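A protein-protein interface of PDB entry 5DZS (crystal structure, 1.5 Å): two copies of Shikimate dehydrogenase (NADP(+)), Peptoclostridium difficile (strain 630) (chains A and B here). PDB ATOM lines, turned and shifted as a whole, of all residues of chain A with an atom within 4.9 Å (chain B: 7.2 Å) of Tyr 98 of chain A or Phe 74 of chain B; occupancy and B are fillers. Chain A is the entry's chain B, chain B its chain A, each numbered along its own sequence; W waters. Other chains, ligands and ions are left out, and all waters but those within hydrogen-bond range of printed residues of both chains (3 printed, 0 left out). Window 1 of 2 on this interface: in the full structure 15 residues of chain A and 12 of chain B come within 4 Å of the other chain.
The side-chain carboxylate of Glu 78 of chain A is in hydrogen-bond range of the backbone NH of Asn 99 of chain A. N of Gly 97 of chain B is in hydrogen-bond range of O of Phe 74 of chain B (2.8 Å). The backbone NH (N) of Ser 76 of chain A sits at hydrogen-bond distance from the backbone carbonyl oxygen (O) of Gly 97 of chain A (2.8 Å). The backbone NH (N) of Asn 86 of chain A is in hydrogen-bond range of the backbone carbonyl oxygen (O) of Tyr 98 of chain A, at 3.0 Å. N of Tyr 98 of chain A is in hydrogen-bond range of O of Thr 87 of chain A, at 2.8 Å. The backbone NH of Leu 89 of chain A lies within hydrogen-bond range of the backbone carbonyl oxygen of Tyr 96 of chain A (2.9 Å).
Among the printed residues, merely in contact across the chains: Pro 77 of chain A with Tyr 96 of chain B (3.5 Å), Tyr 96 of chain A with Pro 77 of chain B (3.5 Å), Pro 77 of chain A with Phe 74 of chain B (3.6 Å), Glu 78 of chain A with Tyr 96 of chain B (3.6 Å), Ser 76 of chain A with Tyr 96 of chain B (3.7 Å), Ser 76 of chain A with Phe 74 of chain B (3.7 Å), Pro 77 of chain A with Met 94 of chain B (3.7 Å), Tyr 96 of chain A with Ile 75 of chain B (3.8 Å), Tyr 98 of chain A with Phe 74 of chain B (3.8 Å), Tyr 98 of chain A with Pro 77 of chain B (3.9 Å), Ile 75 of chain A with Phe 74 of chain B (3.9 Å), Leu 89 of chain A with Pro 77 of chain B (3.998 Å) and Tyr 96 of chain A with Phe 74 of chain B (3.998 Å).
Printed residues of chain B within 4 Å of Ile 75 of chain A: Phe 74. Of the printed residues of chain B, Glu 78 of chain A touches Tyr 96 (3.6 Å). Of the printed residues of chain B, Leu 89 of chain A touches Pro 77. Of the printed residues of chain B, Tyr 96 of chain A touches Phe 74, Ile 75 and Pro 77. Of chain B, only Phe 74 and Pro 77 come within 4 Å of Tyr 98 of chain A. Of the printed residues of chain A, Phe 74 of chain B touches Ile 75, Ser 76, Pro 77, Tyr 96 and Tyr 98. Of the printed residues of chain A, Ile 75 of chain B touches Tyr 96 (3.8 Å). The nearest printed residue of chain B that does not touch Tyr 98 of chain A is Ser 76 of chain B (5.7 Å). The nearest printed residue of chain A that does not touch Phe 74 of chain B is Phe 74 of chain A (4.5 Å).
Of the 15 printed residues of chain B, 5 touch a printed residue of chain A. Printed residues of chain B that touch a printed residue of chain A: Phe 74, Ile 75, Pro 77, Met 94 and Tyr 96. Hydrophobic or aromatic side chains of chain B that line the printed part of chain A: Phe 74, Pro 77, Met 94 and Tyr 96. Hydrophobic or aromatic side chains of chain A that line the printed part of chain B: Pro 77, Leu 89, Tyr 96 and Tyr 98. Among the printed residues, 13 pairs touch across the chains. Among the printed residues, no Asp or Glu carboxylate lies within 4 Å of a Lys or Arg side-chain nitrogen of the other chain.
Ser 76 of chain A touches Phe 74 of chain B, but with the chains exchanged Phe 74 of chain A does not touch Ser 76 of chain B (7.3 Å). Tyr 96 of chain A touches Phe 74 of chain B, but with the chains exchanged Phe 74 of chain A does not touch Tyr 96 of chain B (10.4 Å). Tyr 96 of chain A touches Ile 75 of chain B, but with the chains exchanged Ile 75 of chain A does not touch Tyr 96 of chain B (7.4 Å). Tyr 98 of chain A touches Pro 77 of chain B, but with the chains exchanged Pro 77 of chain A does not touch Tyr 98 of chain B (7.4 Å). Positions printed for both chains: 74, 75, 76, 77, 79, 85, 96, 97 and 98.
Water W1 bridges the backbone carbonyl oxygen (O) of Ile 75 of chain A (2.6 Å) and the backbone carbonyl oxygen (O) of Asp 73 of chain B (2.9 Å). Water W2 bridges the backbone carbonyl oxygen of Ile 75 of chain B (2.7 Å) and the side-chain hydroxyl of Tyr 96 of chain A (3.5 Å). Water W3 bridges the side-chain hydroxyl (OH) of Tyr 96 of chain B (2.9 Å) and the side-chain carboxylate (OE1) of Glu 78 of chain A (3.1 Å).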
ATOM      1  N   PHE A  74      -6.068  13.226  -2.368  1.00  0.00           N
ATOM      2  CA  PHE A  74      -7.042  12.208  -2.089  1.00  0.00           C
ATOM      3  C   PHE A  74      -7.219  11.381  -3.342  1.00  0.00           C
ATOM      4  O   PHE A  74      -7.250  11.936  -4.433  1.00  0.00           O
ATOM      5  CB  PHE A  74      -8.393  12.815  -1.677  1.00  0.00           C
ATOM      6  CG  PHE A  74      -8.294  13.760  -0.521  1.00  0.00           C
ATOM      7  CD1 PHE A  74      -8.126  13.270   0.760  1.00  0.00           C
ATOM      8  CD2 PHE A  74      -8.347  15.139  -0.720  1.00  0.00           C
ATOM      9  CE1 PHE A  74      -8.013  14.144   1.841  1.00  0.00           C
ATOM     10  CE2 PHE A  74      -8.254  15.988   0.355  1.00  0.00           C
ATOM     11  CZ  PHE A  74      -8.074  15.500   1.614  1.00  0.00           C
ATOM     12  N   ILE A  75      -7.310  10.075  -3.180  1.00  0.00           N
ATOM     13  CA  ILE A  75      -7.521   9.137  -4.270  1.00  0.00           C
ATOM     14  C   ILE A  75      -8.786   8.323  -4.031  1.00  0.00           C
ATOM     15  O   ILE A  75      -8.958   7.682  -2.982  1.00  0.00           O
ATOM     16  CB  ILE A  75      -6.306   8.233  -4.468  1.00  0.00           C
ATOM     17  CG1 ILE A  75      -5.066   9.128  -4.718  1.00  0.00           C
ATOM     18  CG2 ILE A  75      -6.551   7.288  -5.634  1.00  0.00           C
ATOM     19  CD1 ILE A  75      -3.764   8.392  -4.890  1.00  0.00           C
ATOM     20  N   SER A  76      -9.695   8.386  -4.995  1.00  0.00           N
ATOM     21  CA  SER A  76     -10.969   7.673  -4.892  1.00  0.00           C
ATOM     22  C   SER A  76     -10.704   6.163  -4.825  1.00  0.00           C
ATOM     23  O   SER A  76      -9.758   5.661  -5.413  1.00  0.00           O
ATOM     24  CB  SER A  76     -11.834   8.116  -6.070  1.00  0.00           C
ATOM     25  OG  SER A  76     -13.137   7.583  -5.992  1.00  0.00           O
ATOM     26  N   PRO A  77     -11.524   5.391  -4.094  1.00  0.00           N
ATOM     27  CA  PRO A  77     -11.264   3.978  -3.908  1.00  0.00           C
ATOM     28  C   PRO A  77     -11.103   3.148  -5.166  1.00  0.00           C
ATOM     29  O   PRO A  77     -10.276   2.264  -5.185  1.00  0.00           O
ATOM     30  CB  PRO A  77     -12.456   3.509  -3.072  1.00  0.00           C
ATOM     31  CG  PRO A  77     -12.897   4.714  -2.314  1.00  0.00           C
ATOM     32  CD  PRO A  77     -12.649   5.863  -3.260  1.00  0.00           C
ATOM     33  N   GLU A  78     -11.868   3.435  -6.220  1.00  0.00           N
ATOM     34  CA  GLU A  78     -11.709   2.668  -7.451  1.00  0.00           C
ATOM     35  C   GLU A  78     -10.331   2.906  -8.086  1.00  0.00           C
ATOM     36  O   GLU A  78      -9.769   2.027  -8.743  1.00  0.00           O
ATOM     37  CB  GLU A  78     -12.838   2.956  -8.467  1.00  0.00           C
ATOM     38  CG  GLU A  78     -12.649   4.159  -9.387  1.00  0.00           C
ATOM     39  CD  GLU A  78     -12.739   5.489  -8.689  1.00  0.00           C
ATOM     40  OE1 GLU A  78     -13.151   5.521  -7.495  1.00  0.00           O
ATOM     41  OE2 GLU A  78     -12.451   6.543  -9.355  1.00  0.00           O
ATOM     42  N   ALA A  79      -9.792   4.114  -7.953  1.00  0.00           N
ATOM     43  CA  ALA A  79      -8.466   4.409  -8.488  1.00  0.00           C
ATOM     44  C   ALA A  79      -7.367   3.723  -7.672  1.00  0.00           C
ATOM     45  O   ALA A  79      -6.351   3.269  -8.218  1.00  0.00           O
ATOM     46  CB  ALA A  79      -8.242   5.918  -8.553  1.00  0.00           C
ATOM     47  N   ALA A  84      -4.115   3.446 -10.583  1.00  0.00           N
ATOM     48  CA  ALA A  84      -3.855   4.493 -11.589  1.00  0.00           C
ATOM     49  C   ALA A  84      -4.973   5.512 -11.544  1.00  0.00           C
ATOM     50  O   ALA A  84      -6.101   5.169 -11.141  1.00  0.00           O
ATOM     51  CB  ALA A  84      -3.802   3.891 -12.969  1.00  0.00           C
ATOM     52  N   VAL A  85      -4.658   6.726 -12.004  1.00  0.00           N
ATOM     53  CA  VAL A  85      -5.586   7.835 -12.066  1.00  0.00           C
ATOM     54  C   VAL A  85      -5.639   8.415 -13.466  1.00  0.00           C
ATOM     55  O   VAL A  85      -4.589   8.649 -14.064  1.00  0.00           O
ATOM     56  CB  VAL A  85      -5.162   8.917 -11.055  1.00  0.00           C
ATOM     57  CG1 VAL A  85      -5.784  10.290 -11.340  1.00  0.00           C
ATOM     58  CG2 VAL A  85      -5.513   8.440  -9.660  1.00  0.00           C
ATOM     59  N   ASN A  86      -6.841   8.649 -14.010  1.00  0.00           N
ATOM     60  CA  ASN A  86      -6.975   9.344 -15.296  1.00  0.00           C
ATOM     61  C   ASN A  86      -7.803  10.613 -15.235  1.00  0.00           C
ATOM     62  O   ASN A  86      -7.970  11.257 -16.268  1.00  0.00           O
ATOM     63  CB  ASN A  86      -7.516   8.418 -16.371  1.00  0.00           C
ATOM     64  CG  ASN A  86      -8.980   8.131 -16.218  1.00  0.00           C
ATOM     65  OD1 ASN A  86      -9.622   8.474 -15.226  1.00  0.00           O
ATOM     66  ND2 ASN A  86      -9.534   7.498 -17.237  1.00  0.00           N
ATOM     67  N   THR A  87      -8.282  10.988 -14.048  1.00  0.00           N
ATOM     68  CA  THR A  87      -9.149  12.166 -13.888  1.00  0.00           C
ATOM     69  C   THR A  87      -8.778  12.824 -12.568  1.00  0.00           C
ATOM     70  O   THR A  87      -8.785  12.156 -11.532  1.00  0.00           O
ATOM     71  CB  THR A  87     -10.634  11.757 -13.914  1.00  0.00           C
ATOM     72  OG1 THR A  87     -10.943  11.125 -15.173  1.00  0.00           O
ATOM     73  CG2 THR A  87     -11.559  12.947 -13.713  1.00  0.00           C
ATOM     74  N   LEU A  89      -9.508  16.332 -10.057  1.00  0.00           N
ATOM     75  CA  LEU A  89     -10.395  17.453  -9.730  1.00  0.00           C
ATOM     76  C   LEU A  89      -9.694  18.323  -8.687  1.00  0.00           C
ATOM     77  O   LEU A  89      -9.186  17.815  -7.681  1.00  0.00           O
ATOM     78  CB  LEU A  89     -11.697  16.937  -9.142  1.00  0.00           C
ATOM     79  CG  LEU A  89     -12.654  17.975  -8.540  1.00  0.00           C
ATOM     80  CD1 LEU A  89     -13.131  19.052  -9.501  1.00  0.00           C
ATOM     81  CD2 LEU A  89     -13.847  17.244  -7.945  1.00  0.00           C
ATOM     82  N   TYR A  96      -7.952  15.710  -6.106  1.00  0.00           N
ATOM     83  CA  TYR A  96      -8.651  14.436  -5.962  1.00  0.00           C
ATOM     84  C   TYR A  96      -8.478  13.645  -7.231  1.00  0.00           C
ATOM     85  O   TYR A  96      -8.730  14.165  -8.337  1.00  0.00           O
ATOM     86  CB  TYR A  96     -10.147  14.663  -5.741  1.00  0.00           C
ATOM     87  CG  TYR A  96     -10.500  15.331  -4.425  1.00  0.00           C
ATOM     88  CD1 TYR A  96     -10.272  16.684  -4.214  1.00  0.00           C
ATOM     89  CD2 TYR A  96     -11.106  14.613  -3.423  1.00  0.00           C
ATOM     90  CE1 TYR A  96     -10.583  17.268  -3.004  1.00  0.00           C
ATOM     91  CE2 TYR A  96     -11.445  15.206  -2.237  1.00  0.00           C
ATOM     92  CZ  TYR A  96     -11.167  16.519  -2.027  1.00  0.00           C
ATOM     93  OH  TYR A  96     -11.518  17.145  -0.828  1.00  0.00           O
ATOM     94  N   GLY A  97      -8.057  12.410  -7.100  1.00  0.00           N
ATOM     95  CA  GLY A  97      -7.852  11.511  -8.228  1.00  0.00           C
ATOM     96  C   GLY A  97      -8.918  10.439  -8.361  1.00  0.00           C
ATOM     97  O   GLY A  97      -9.287   9.793  -7.359  1.00  0.00           O
ATOM     98  N   TYR A  98      -9.350  10.203  -9.602  1.00  0.00           N
ATOM     99  CA  TYR A  98     -10.362   9.217  -9.944  1.00  0.00           C
ATOM    100  C   TYR A  98      -9.907   8.418 -11.146  1.00  0.00           C
ATOM    101  O   TYR A  98      -8.963   8.812 -11.848  1.00  0.00           O
ATOM    102  CB  TYR A  98     -11.697   9.907 -10.312  1.00  0.00           C
ATOM    103  CG  TYR A  98     -12.227  10.858  -9.279  1.00  0.00           C
ATOM    104  CD1 TYR A  98     -11.751  12.164  -9.178  1.00  0.00           C
ATOM    105  CD2 TYR A  98     -13.208  10.473  -8.396  1.00  0.00           C
ATOM    106  CE1 TYR A  98     -12.218  13.018  -8.219  1.00  0.00           C
ATOM    107  CE2 TYR A  98     -13.720  11.363  -7.462  1.00  0.00           C
ATOM    108  CZ  TYR A  98     -13.212  12.653  -7.395  1.00  0.00           C
ATOM    109  OH  TYR A  98     -13.705  13.543  -6.443  1.00  0.00           O
ATOM    110  N   ASN A  99     -10.575   7.307 -11.402  1.00  0.00           N
ATOM    111  CA  ASN A  99     -10.266   6.514 -12.578  1.00  0.00           C
ATOM    112  C   ASN A  99     -11.530   6.090 -13.257  1.00  0.00           C
ATOM    113  O   ASN A  99     -12.303   5.281 -12.712  1.00  0.00           O
ATOM    114  CB  ASN A  99      -9.417   5.317 -12.217  1.00  0.00           C
ATOM    115  CG  ASN A  99      -8.936   4.584 -13.452  1.00  0.00           C
ATOM    116  OD1 ASN A  99      -9.744   4.280 -14.345  1.00  0.00           O
ATOM    117  ND2 ASN A  99      -7.656   4.299 -13.517  1.00  0.00           N
ATOM    118  N   THR A 100     -11.761   6.609 -14.449  1.00  0.00           N
ATOM    119  CA  THR A 100     -12.920   6.203 -15.185  1.00  0.00           C
ATOM    120  C   THR A 100     -12.630   5.016 -16.141  1.00  0.00           C
ATOM    121  O   THR A 100     -13.537   4.651 -16.922  1.00  0.00           O
ATOM    122  CB  THR A 100     -13.360   7.320 -16.037  1.00  0.00           C
ATOM    123  OG1 THR A 100     -12.307   7.533 -17.007  1.00  0.00           O
ATOM    124  CG2 THR A 100     -13.661   8.598 -15.201  1.00  0.00           C
ATOM    125  N   ILE A 246     -17.988  14.129 -12.710  1.00  0.00           N
ATOM    126  CA  ILE A 246     -17.149  14.309 -11.528  1.00  0.00           C
ATOM    127  C   ILE A 246     -16.769  15.777 -11.306  1.00  0.00           C
ATOM    128  O   ILE A 246     -16.895  16.310 -10.198  1.00  0.00           O
ATOM    129  CB  ILE A 246     -15.869  13.461 -11.653  1.00  0.00           C
ATOM    130  CG1 ILE A 246     -16.235  11.971 -11.533  1.00  0.00           C
ATOM    131  CG2 ILE A 246     -14.861  13.862 -10.565  1.00  0.00           C
ATOM    132  CD1 ILE A 246     -15.138  11.038 -11.962  1.00  0.00           C
ATOM    133  N   MET B  69     -17.825  10.408   9.582  1.00  0.00           N
ATOM    134  CA  MET B  69     -16.832  10.657   8.512  1.00  0.00           C
ATOM    135  C   MET B  69     -15.564   9.846   8.694  1.00  0.00           C
ATOM    136  O   MET B  69     -15.045   9.288   7.712  1.00  0.00           O
ATOM    137  CB  MET B  69     -16.507  12.163   8.372  1.00  0.00           C
ATOM    138  CG  MET B  69     -17.745  12.996   8.054  1.00  0.00           C
ATOM    139  SD  MET B  69     -17.420  14.752   7.945  1.00  0.00           S
ATOM    140  CE  MET B  69     -16.258  14.728   6.595  1.00  0.00           C
ATOM    141  N   TYR B  71     -15.040   6.946   9.725  1.00  0.00           N
ATOM    142  CA  TYR B  71     -15.196   5.513   9.439  1.00  0.00           C
ATOM    143  C   TYR B  71     -15.278   5.200   7.948  1.00  0.00           C
ATOM    144  O   TYR B  71     -15.310   4.035   7.572  1.00  0.00           O
ATOM    145  CB  TYR B  71     -16.436   4.953  10.118  1.00  0.00           C
ATOM    146  CG  TYR B  71     -16.345   5.048  11.644  1.00  0.00           C
ATOM    147  CD1 TYR B  71     -15.667   4.097  12.373  1.00  0.00           C
ATOM    148  CD2 TYR B  71     -16.946   6.084  12.326  1.00  0.00           C
ATOM    149  CE1 TYR B  71     -15.565   4.184  13.747  1.00  0.00           C
ATOM    150  CE2 TYR B  71     -16.846   6.187  13.712  1.00  0.00           C
ATOM    151  CZ  TYR B  71     -16.199   5.218  14.415  1.00  0.00           C
ATOM    152  OH  TYR B  71     -16.076   5.342  15.788  1.00  0.00           O
ATOM    153  N   LEU B  72     -15.270   6.229   7.106  1.00  0.00           N
ATOM    154  CA  LEU B  72     -15.448   6.025   5.664  1.00  0.00           C
ATOM    155  C   LEU B  72     -14.131   5.965   4.932  1.00  0.00           C
ATOM    156  O   LEU B  72     -13.103   6.407   5.429  1.00  0.00           O
ATOM    157  CB  LEU B  72     -16.316   7.151   5.128  1.00  0.00           C
ATOM    158  CG  LEU B  72     -17.639   7.405   5.882  1.00  0.00           C
ATOM    159  CD1 LEU B  72     -18.439   8.517   5.241  1.00  0.00           C
ATOM    160  CD2 LEU B  72     -18.440   6.122   6.008  1.00  0.00           C
ATOM    161  N   ASP B  73     -14.161   5.403   3.729  1.00  0.00           N
ATOM    162  CA  ASP B  73     -12.973   5.262   2.902  1.00  0.00           C
ATOM    163  C   ASP B  73     -12.642   6.469   2.037  1.00  0.00           C
ATOM    164  O   ASP B  73     -11.461   6.651   1.686  1.00  0.00           O
ATOM    165  CB  ASP B  73     -13.113   4.017   2.053  1.00  0.00           C
ATOM    166  CG  ASP B  73     -13.284   2.786   2.908  1.00  0.00           C
ATOM    167  OD1 ASP B  73     -12.270   2.406   3.566  1.00  0.00           O
ATOM    168  OD2 ASP B  73     -14.376   2.200   2.958  1.00  0.00           O
ATOM    169  N   PHE B  74     -13.636   7.285   1.716  1.00  0.00           N
ATOM    170  CA  PHE B  74     -13.436   8.461   0.840  1.00  0.00           C
ATOM    171  C   PHE B  74     -14.464   9.506   1.205  1.00  0.00           C
ATOM    172  O   PHE B  74     -15.639   9.168   1.411  1.00  0.00           O
ATOM    173  CB  PHE B  74     -13.643   8.038  -0.612  1.00  0.00           C
ATOM    174  CG  PHE B  74     -13.488   9.152  -1.612  1.00  0.00           C
ATOM    175  CD1 PHE B  74     -12.249   9.604  -1.962  1.00  0.00           C
ATOM    176  CD2 PHE B  74     -14.609   9.761  -2.164  1.00  0.00           C
ATOM    177  CE1 PHE B  74     -12.081  10.627  -2.897  1.00  0.00           C
ATOM    178  CE2 PHE B  74     -14.465  10.788  -3.069  1.00  0.00           C
ATOM    179  CZ  PHE B  74     -13.214  11.216  -3.428  1.00  0.00           C
ATOM    180  N   ILE B  75     -14.017  10.737   1.346  1.00  0.00           N
ATOM    181  CA  ILE B  75     -14.868  11.872   1.631  1.00  0.00           C
ATOM    182  C   ILE B  75     -14.835  12.792   0.401  1.00  0.00           C
ATOM    183  O   ILE B  75     -13.796  13.273  -0.004  1.00  0.00           O
ATOM    184  CB  ILE B  75     -14.381  12.630   2.870  1.00  0.00           C
ATOM    185  CG1 ILE B  75     -14.306  11.712   4.106  1.00  0.00           C
ATOM    186  CG2 ILE B  75     -15.277  13.838   3.126  1.00  0.00           C
ATOM    187  CD1 ILE B  75     -15.615  11.112   4.538  1.00  0.00           C
ATOM    188  N   SER B  76     -16.006  13.023  -0.183  1.00  0.00           N
ATOM    189  CA  SER B  76     -16.096  13.908  -1.335  1.00  0.00           C
ATOM    190  C   SER B  76     -15.660  15.325  -1.001  1.00  0.00           C
ATOM    191  O   SER B  76     -15.630  15.748   0.156  1.00  0.00           O
ATOM    192  CB  SER B  76     -17.522  13.935  -1.868  1.00  0.00           C
ATOM    193  OG  SER B  76     -18.391  14.606  -0.979  1.00  0.00           O
ATOM    194  N   PRO B  77     -15.284  16.090  -2.031  1.00  0.00           N
ATOM    195  CA  PRO B  77     -14.895  17.466  -1.791  1.00  0.00           C
ATOM    196  C   PRO B  77     -15.913  18.322  -1.030  1.00  0.00           C
ATOM    197  O   PRO B  77     -15.535  19.065  -0.118  1.00  0.00           O
ATOM    198  CB  PRO B  77     -14.660  18.005  -3.195  1.00  0.00           C
ATOM    199  CG  PRO B  77     -14.302  16.840  -3.994  1.00  0.00           C
ATOM    200  CD  PRO B  77     -14.990  15.654  -3.406  1.00  0.00           C
ATOM    201  N   ALA B  79     -18.364  17.277   1.032  1.00  0.00           N
ATOM    202  CA  ALA B  79     -18.473  16.823   2.393  1.00  0.00           C
ATOM    203  C   ALA B  79     -17.287  17.295   3.192  1.00  0.00           C
ATOM    204  O   ALA B  79     -17.435  17.711   4.336  1.00  0.00           O
ATOM    205  CB  ALA B  79     -18.610  15.310   2.459  1.00  0.00           C
ATOM    206  N   VAL B  85     -21.192  14.545   6.645  1.00  0.00           N
ATOM    207  CA  VAL B  85     -21.679  13.585   5.658  1.00  0.00           C
ATOM    208  C   VAL B  85     -23.129  13.234   5.954  1.00  0.00           C
ATOM    209  O   VAL B  85     -23.430  12.892   7.087  1.00  0.00           O
ATOM    210  CB  VAL B  85     -20.815  12.309   5.624  1.00  0.00           C
ATOM    211  CG1 VAL B  85     -21.527  11.129   4.979  1.00  0.00           C
ATOM    212  CG2 VAL B  85     -19.518  12.603   4.872  1.00  0.00           C
ATOM    213  N   MET B  94     -16.214  -0.550  -0.352  1.00  0.00           N
ATOM    214  CA  MET B  94     -15.690   0.723   0.134  1.00  0.00           C
ATOM    215  C   MET B  94     -16.846   1.692   0.341  1.00  0.00           C
ATOM    216  O   MET B  94     -17.837   1.670  -0.408  1.00  0.00           O
ATOM    217  CB  MET B  94     -14.700   1.309  -0.878  1.00  0.00           C
ATOM    218  CG  MET B  94     -13.421   0.506  -1.071  1.00  0.00           C
ATOM    219  SD  MET B  94     -12.347   0.571   0.375  1.00  0.00           S
ATOM    220  CE  MET B  94     -11.153  -0.728   0.097  1.00  0.00           C
ATOM    221  N   LEU B  95     -16.705   2.550   1.346  1.00  0.00           N
ATOM    222  CA  LEU B  95     -17.728   3.530   1.691  1.00  0.00           C
ATOM    223  C   LEU B  95     -17.298   4.942   1.322  1.00  0.00           C
ATOM    224  O   LEU B  95     -16.224   5.424   1.693  1.00  0.00           O
ATOM    225  CB  LEU B  95     -18.093   3.476   3.186  1.00  0.00           C
ATOM    226  CG  LEU B  95     -18.679   2.183   3.695  1.00  0.00           C
ATOM    227  CD1 LEU B  95     -18.948   2.289   5.192  1.00  0.00           C
ATOM    228  CD2 LEU B  95     -19.949   1.843   2.948  1.00  0.00           C
ATOM    229  N   TYR B  96     -18.183   5.601   0.566  1.00  0.00           N
ATOM    230  CA  TYR B  96     -17.966   6.947   0.057  1.00  0.00           C
ATOM    231  C   TYR B  96     -18.928   7.902   0.739  1.00  0.00           C
ATOM    232  O   TYR B  96     -20.141   7.624   0.795  1.00  0.00           O
ATOM    233  CB  TYR B  96     -18.251   6.987  -1.442  1.00  0.00           C
ATOM    234  CG  TYR B  96     -17.402   6.136  -2.378  1.00  0.00           C
ATOM    235  CD1 TYR B  96     -17.383   4.739  -2.313  1.00  0.00           C
ATOM    236  CD2 TYR B  96     -16.730   6.729  -3.427  1.00  0.00           C
ATOM    237  CE1 TYR B  96     -16.647   4.000  -3.217  1.00  0.00           C
ATOM    238  CE2 TYR B  96     -16.011   5.989  -4.336  1.00  0.00           C
ATOM    239  CZ  TYR B  96     -15.970   4.628  -4.213  1.00  0.00           C
ATOM    240  OH  TYR B  96     -15.243   3.874  -5.116  1.00  0.00           O
ATOM    241  N   GLY B  97     -18.418   9.017   1.241  1.00  0.00           N
ATOM    242  CA  GLY B  97     -19.248   9.980   1.925  1.00  0.00           C
ATOM    243  C   GLY B  97     -19.484  11.256   1.129  1.00  0.00           C
ATOM    244  O   GLY B  97     -18.541  11.886   0.609  1.00  0.00           O
ATOM    245  N   TYR B  98     -20.751  11.638   1.086  1.00  0.00           N
ATOM    246  CA  TYR B  98     -21.247  12.816   0.340  1.00  0.00           C
ATOM    247  C   TYR B  98     -22.123  13.676   1.223  1.00  0.00           C
ATOM    248  O   TYR B  98     -22.578  13.240   2.294  1.00  0.00           O
ATOM    249  CB  TYR B  98     -22.084  12.386  -0.877  1.00  0.00           C
ATOM    250  CG  TYR B  98     -21.312  11.515  -1.872  1.00  0.00           C
ATOM    251  CD1 TYR B  98     -20.490  12.102  -2.806  1.00  0.00           C
ATOM    252  CD2 TYR B  98     -21.379  10.110  -1.840  1.00  0.00           C
ATOM    253  CE1 TYR B  98     -19.777  11.333  -3.695  1.00  0.00           C
ATOM    254  CE2 TYR B  98     -20.662   9.353  -2.725  1.00  0.00           C
ATOM    255  CZ  TYR B  98     -19.848   9.967  -3.627  1.00  0.00           C
ATOM    256  OH  TYR B  98     -19.101   9.210  -4.525  1.00  0.00           O
HETATM  257  O   HOH W   1     -10.158   6.649  -0.948  1.00  0.00           O
HETATM  258  O   HOH W   2     -11.587  14.313   1.184  1.00  0.00           O
HETATM  259  O   HOH W   3     -16.159   4.853  -7.716  1.00  0.00           O
